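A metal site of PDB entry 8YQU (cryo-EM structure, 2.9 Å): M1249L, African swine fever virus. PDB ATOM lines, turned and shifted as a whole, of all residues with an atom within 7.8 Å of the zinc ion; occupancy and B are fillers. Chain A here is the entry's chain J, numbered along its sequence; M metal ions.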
ATOM      1  N   SER A 847      13.211 -28.780 -10.394  1.00  0.00           N
ATOM      2  CA  SER A 847      12.832 -28.447  -9.034  1.00  0.00           C
ATOM      3  C   SER A 847      12.551 -26.971  -8.834  1.00  0.00           C
ATOM      4  O   SER A 847      11.876 -26.607  -7.871  1.00  0.00           O
ATOM      5  CB  SER A 847      13.925 -28.901  -8.067  1.00  0.00           C
ATOM      6  OG  SER A 847      15.153 -28.253  -8.350  1.00  0.00           O
ATOM      7  N   THR A 848      13.045 -26.107  -9.730  1.00  0.00           N
ATOM      8  CA  THR A 848      12.790 -24.676  -9.627  1.00  0.00           C
ATOM      9  C   THR A 848      11.353 -24.302  -9.975  1.00  0.00           C
ATOM     10  O   THR A 848      10.871 -23.275  -9.495  1.00  0.00           O
ATOM     11  CB  THR A 848      13.745 -23.902 -10.537  1.00  0.00           C
ATOM     12  OG1 THR A 848      13.472 -24.241 -11.912  1.00  0.00           O
ATOM     13  CG2 THR A 848      15.184 -24.265 -10.217  1.00  0.00           C
ATOM     14  N   LEU A 849      10.669 -25.113 -10.786  1.00  0.00           N
ATOM     15  CA  LEU A 849       9.302 -24.820 -11.189  1.00  0.00           C
ATOM     16  C   LEU A 849       8.257 -25.640 -10.447  1.00  0.00           C
ATOM     17  O   LEU A 849       7.129 -25.183 -10.268  1.00  0.00           O
ATOM     18  CB  LEU A 849       9.126 -25.035 -12.695  1.00  0.00           C
ATOM     19  CG  LEU A 849       9.813 -24.046 -13.629  1.00  0.00           C
ATOM     20  CD1 LEU A 849       9.560 -24.420 -15.081  1.00  0.00           C
ATOM     21  CD2 LEU A 849       9.337 -22.624 -13.347  1.00  0.00           C
ATOM     22  N   TYR A 850       8.607 -26.856 -10.013  1.00  0.00           N
ATOM     23  CA  TYR A 850       7.665 -27.746  -9.350  1.00  0.00           C
ATOM     24  C   TYR A 850       8.319 -28.353  -8.121  1.00  0.00           C
ATOM     25  O   TYR A 850       9.531 -28.544  -8.073  1.00  0.00           O
ATOM     26  CB  TYR A 850       7.190 -28.856 -10.304  1.00  0.00           C
ATOM     27  CG  TYR A 850       6.575 -28.336 -11.584  1.00  0.00           C
ATOM     28  CD1 TYR A 850       5.244 -27.956 -11.627  1.00  0.00           C
ATOM     29  CD2 TYR A 850       7.330 -28.212 -12.738  1.00  0.00           C
ATOM     30  CE1 TYR A 850       4.687 -27.467 -12.795  1.00  0.00           C
ATOM     31  CE2 TYR A 850       6.781 -27.733 -13.912  1.00  0.00           C
ATOM     32  CZ  TYR A 850       5.449 -27.364 -13.925  1.00  0.00           C
ATOM     33  OH  TYR A 850       4.900 -26.885 -15.085  1.00  0.00           O
ATOM     34  N   ASP A 851       7.492 -28.659  -7.125  1.00  0.00           N
ATOM     35  CA  ASP A 851       7.986 -29.210  -5.863  1.00  0.00           C
ATOM     36  C   ASP A 851       8.002 -30.736  -5.950  1.00  0.00           C
ATOM     37  O   ASP A 851       7.824 -31.330  -7.025  1.00  0.00           O
ATOM     38  CB  ASP A 851       7.134 -28.718  -4.694  1.00  0.00           C
ATOM     39  CG  ASP A 851       5.683 -29.157  -4.807  1.00  0.00           C
ATOM     40  OD1 ASP A 851       5.206 -29.363  -5.940  1.00  0.00           O
ATOM     41  OD2 ASP A 851       5.025 -29.286  -3.759  1.00  0.00           O
ATOM     42  N   GLU A 852       8.227 -31.397  -4.818  1.00  0.00           N
ATOM     43  CA  GLU A 852       8.318 -32.847  -4.782  1.00  0.00           C
ATOM     44  C   GLU A 852       6.968 -33.536  -4.964  1.00  0.00           C
ATOM     45  O   GLU A 852       6.941 -34.764  -5.103  1.00  0.00           O
ATOM     46  CB  GLU A 852       8.952 -33.301  -3.458  1.00  0.00           C
ATOM     47  CG  GLU A 852      10.453 -33.069  -3.387  1.00  0.00           C
ATOM     48  CD  GLU A 852      11.030 -33.381  -2.023  1.00  0.00           C
ATOM     49  OE1 GLU A 852      10.243 -33.518  -1.066  1.00  0.00           O
ATOM     50  OE2 GLU A 852      12.263 -33.497  -1.912  1.00  0.00           O
ATOM     51  N   LEU A 855       3.354 -30.006  -7.830  1.00  0.00           N
ATOM     52  CA  LEU A 855       2.611 -28.767  -7.957  1.00  0.00           C
ATOM     53  C   LEU A 855       3.539 -27.602  -8.323  1.00  0.00           C
ATOM     54  O   LEU A 855       4.716 -27.612  -7.955  1.00  0.00           O
ATOM     55  CB  LEU A 855       1.878 -28.443  -6.659  1.00  0.00           C
ATOM     56  CG  LEU A 855       0.753 -29.404  -6.263  1.00  0.00           C
ATOM     57  CD1 LEU A 855       0.249 -29.088  -4.858  1.00  0.00           C
ATOM     58  CD2 LEU A 855      -0.377 -29.347  -7.271  1.00  0.00           C
ATOM     59  N   PRO A 856       3.049 -26.617  -9.055  1.00  0.00           N
ATOM     60  CA  PRO A 856       3.885 -25.456  -9.387  1.00  0.00           C
ATOM     61  C   PRO A 856       4.154 -24.598  -8.164  1.00  0.00           C
ATOM     62  O   PRO A 856       3.398 -24.566  -7.195  1.00  0.00           O
ATOM     63  CB  PRO A 856       3.049 -24.697 -10.419  1.00  0.00           C
ATOM     64  CG  PRO A 856       1.648 -25.084 -10.134  1.00  0.00           C
ATOM     65  CD  PRO A 856       1.702 -26.508  -9.642  1.00  0.00           C
ATOM     66  N   HIS A 857       5.283 -23.887  -8.218  1.00  0.00           N
ATOM     67  CA  HIS A 857       5.653 -22.974  -7.141  1.00  0.00           C
ATOM     68  C   HIS A 857       4.921 -21.644  -7.284  1.00  0.00           C
ATOM     69  O   HIS A 857       4.728 -21.149  -8.389  1.00  0.00           O
ATOM     70  CB  HIS A 857       7.164 -22.735  -7.128  1.00  0.00           C
ATOM     71  CG  HIS A 857       7.955 -23.892  -6.592  1.00  0.00           C
ATOM     72  ND1 HIS A 857       7.771 -24.391  -5.328  1.00  0.00           N
ATOM     73  CD2 HIS A 857       8.947 -24.627  -7.158  1.00  0.00           C
ATOM     74  CE1 HIS A 857       8.604 -25.403  -5.134  1.00  0.00           C
ATOM     75  NE2 HIS A 857       9.335 -25.560  -6.233  1.00  0.00           N
ATOM     76  N   LYS A 858       4.518 -21.079  -6.142  1.00  0.00           N
ATOM     77  CA  LYS A 858       3.884 -19.759  -6.083  1.00  0.00           C
ATOM     78  C   LYS A 858       4.649 -18.951  -5.043  1.00  0.00           C
ATOM     79  O   LYS A 858       4.284 -18.954  -3.861  1.00  0.00           O
ATOM     80  CB  LYS A 858       2.407 -19.875  -5.746  1.00  0.00           C
ATOM     81  CG  LYS A 858       1.560 -20.550  -6.822  1.00  0.00           C
ATOM     82  CD  LYS A 858       0.082 -20.406  -6.522  1.00  0.00           C
ATOM     83  CE  LYS A 858      -0.763 -21.074  -7.591  1.00  0.00           C
ATOM     84  NZ  LYS A 858      -0.647 -22.551  -7.547  1.00  0.00           N
ATOM     85  N   TRP A 859       5.697 -18.254  -5.482  1.00  0.00           N
ATOM     86  CA  TRP A 859       6.529 -17.483  -4.578  1.00  0.00           C
ATOM     87  C   TRP A 859       5.793 -16.224  -4.145  1.00  0.00           C
ATOM     88  O   TRP A 859       5.896 -15.184  -4.805  1.00  0.00           O
ATOM     89  CB  TRP A 859       7.857 -17.123  -5.233  1.00  0.00           C
ATOM     90  CG  TRP A 859       8.566 -18.298  -5.835  1.00  0.00           C
ATOM     91  CD1 TRP A 859       8.702 -18.576  -7.163  1.00  0.00           C
ATOM     92  CD2 TRP A 859       9.225 -19.347  -5.130  1.00  0.00           C
ATOM     93  NE1 TRP A 859       9.412 -19.735  -7.326  1.00  0.00           N
ATOM     94  CE2 TRP A 859       9.753 -20.231  -6.095  1.00  0.00           C
ATOM     95  CE3 TRP A 859       9.438 -19.632  -3.774  1.00  0.00           C
ATOM     96  CZ2 TRP A 859      10.457 -21.373  -5.754  1.00  0.00           C
ATOM     97  CZ3 TRP A 859      10.143 -20.767  -3.440  1.00  0.00           C
ATOM     98  CH2 TRP A 859      10.644 -21.631  -4.420  1.00  0.00           C
ATOM     99  N   ARG A 897       9.207 -17.045  -0.409  1.00  0.00           N
ATOM    100  CA  ARG A 897       8.704 -18.334   0.027  1.00  0.00           C
ATOM    101  C   ARG A 897       7.482 -18.732  -0.794  1.00  0.00           C
ATOM    102  O   ARG A 897       6.655 -17.883  -1.144  1.00  0.00           O
ATOM    103  CB  ARG A 897       8.355 -18.330   1.528  1.00  0.00           C
ATOM    104  CG  ARG A 897       8.065 -19.699   2.100  1.00  0.00           C
ATOM    105  CD  ARG A 897       7.903 -19.645   3.606  1.00  0.00           C
ATOM    106  NE  ARG A 897       9.176 -19.440   4.291  1.00  0.00           N
ATOM    107  CZ  ARG A 897       9.964 -20.419   4.712  1.00  0.00           C
ATOM    108  NH1 ARG A 897       9.636 -21.689   4.531  1.00  0.00           N
ATOM    109  NH2 ARG A 897      11.102 -20.118   5.312  1.00  0.00           N
ATOM    110  N   CYS A 898       7.392 -20.022  -1.108  1.00  0.00           N
ATOM    111  CA  CYS A 898       6.261 -20.564  -1.837  1.00  0.00           C
ATOM    112  C   CYS A 898       5.088 -20.762  -0.885  1.00  0.00           C
ATOM    113  O   CYS A 898       5.252 -21.287   0.217  1.00  0.00           O
ATOM    114  CB  CYS A 898       6.633 -21.884  -2.505  1.00  0.00           C
ATOM    115  SG  CYS A 898       5.336 -22.599  -3.527  1.00  0.00           S
ATOM    116  N   SER A 899       3.895 -20.345  -1.317  1.00  0.00           N
ATOM    117  CA  SER A 899       2.677 -20.485  -0.532  1.00  0.00           C
ATOM    118  C   SER A 899       2.010 -21.841  -0.705  1.00  0.00           C
ATOM    119  O   SER A 899       0.834 -21.991  -0.363  1.00  0.00           O
ATOM    120  CB  SER A 899       1.700 -19.366  -0.882  1.00  0.00           C
ATOM    121  OG  SER A 899       1.268 -19.474  -2.226  1.00  0.00           O
ATOM    122  N   VAL A 900       2.735 -22.835  -1.225  1.00  0.00           N
ATOM    123  CA  VAL A 900       2.175 -24.169  -1.428  1.00  0.00           C
ATOM    124  C   VAL A 900       3.020 -25.184  -0.666  1.00  0.00           C
ATOM    125  O   VAL A 900       2.520 -25.863   0.235  1.00  0.00           O
ATOM    126  CB  VAL A 900       2.101 -24.517  -2.922  1.00  0.00           C
ATOM    127  CG1 VAL A 900       1.661 -25.957  -3.102  1.00  0.00           C
ATOM    128  CG2 VAL A 900       1.158 -23.576  -3.643  1.00  0.00           C
ATOM    129  N   CYS A 901       4.297 -25.293  -1.021  1.00  0.00           N
ATOM    130  CA  CYS A 901       5.191 -26.253  -0.387  1.00  0.00           C
ATOM    131  C   CYS A 901       5.992 -25.654   0.762  1.00  0.00           C
ATOM    132  O   CYS A 901       6.672 -26.409   1.476  1.00  0.00           O
ATOM    133  CB  CYS A 901       6.149 -26.839  -1.434  1.00  0.00           C
ATOM    134  SG  CYS A 901       7.113 -25.606  -2.335  1.00  0.00           S
ATOM    135  N   HIS A 902       5.940 -24.336   0.948  1.00  0.00           N
ATOM    136  CA  HIS A 902       6.605 -23.651   2.055  1.00  0.00           C
ATOM    137  C   HIS A 902       8.112 -23.937   2.072  1.00  0.00           C
ATOM    138  O   HIS A 902       8.660 -24.512   3.013  1.00  0.00           O
ATOM    139  CB  HIS A 902       5.962 -24.024   3.401  1.00  0.00           C
ATOM    140  CG  HIS A 902       4.509 -23.703   3.485  1.00  0.00           C
ATOM    141  ND1 HIS A 902       3.518 -24.639   3.237  1.00  0.00           N
ATOM    142  CD2 HIS A 902       3.865 -22.548   3.772  1.00  0.00           C
ATOM    143  CE1 HIS A 902       2.334 -24.070   3.382  1.00  0.00           C
ATOM    144  NE2 HIS A 902       2.513 -22.800   3.707  1.00  0.00           N
ATOM    145  N   VAL A 903       8.766 -23.526   0.992  1.00  0.00           N
ATOM    146  CA  VAL A 903      10.213 -23.652   0.856  1.00  0.00           C
ATOM    147  C   VAL A 903      10.779 -22.313   0.418  1.00  0.00           C
ATOM    148  O   VAL A 903      10.122 -21.550  -0.298  1.00  0.00           O
ATOM    149  CB  VAL A 903      10.611 -24.770  -0.137  1.00  0.00           C
ATOM    150  CG1 VAL A 903      10.335 -24.348  -1.573  1.00  0.00           C
ATOM    151  CG2 VAL A 903      12.068 -25.160   0.034  1.00  0.00           C
ATOM    152  N   LEU A 911      15.543 -29.895  -2.874  1.00  0.00           N
ATOM    153  CA  LEU A 911      14.524 -30.835  -3.311  1.00  0.00           C
ATOM    154  C   LEU A 911      15.159 -31.931  -4.172  1.00  0.00           C
ATOM    155  O   LEU A 911      16.086 -31.676  -4.935  1.00  0.00           O
ATOM    156  CB  LEU A 911      13.428 -30.128  -4.102  1.00  0.00           C
ATOM    157  CG  LEU A 911      12.586 -29.103  -3.343  1.00  0.00           C
ATOM    158  CD1 LEU A 911      11.654 -28.371  -4.295  1.00  0.00           C
ATOM    159  CD2 LEU A 911      11.801 -29.765  -2.226  1.00  0.00           C
HETATM  160 ZN    ZN M   1       5.875 -24.773  -4.081  1.00  0.00          ZN
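SG of Cys 901 binds the zinc ion (2.3 Å).
ND1 of His 857 is bound to the zinc ion (2.3 Å).
The side-chain sulfur (SG) of Cys 898 binds the zinc ion (2.3 Å).
O of Pro 856 touches the zinc ion, 3.98 Å away.
CB of Val 900 touches the zinc ion, 3.96 Å away.
Of the 19 residues printed, 5 come within 4 Å of the zinc ion.
The backbone NH (N) of His 857 is in hydrogen-bond range of the backbone carbonyl oxygen (O) of Leu 849 (3.0 Å).
The backbone carbonyl oxygen of Ser 847 lies within hydrogen-bond range of a ring nitrogen (NE2) of His 857 (3.2 Å).
The side-chain sulfur of Cys 898 sits close to the backbone NH of Val 900 (3.5 Å).
The backbone NH (N) of Lys 858 lies close to the side-chain sulfur (SG) of Cys 898, at 3.1 Å.
The backbone NH (N) of Cys 898 sits at hydrogen-bond distance from the backbone carbonyl oxygen (O) of Val 903 (3.2 Å).
The backbone carbonyl oxygen (O) of Val 900 sits at hydrogen-bond distance from a ring nitrogen (ND1) of His 902 (3.4 Å).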
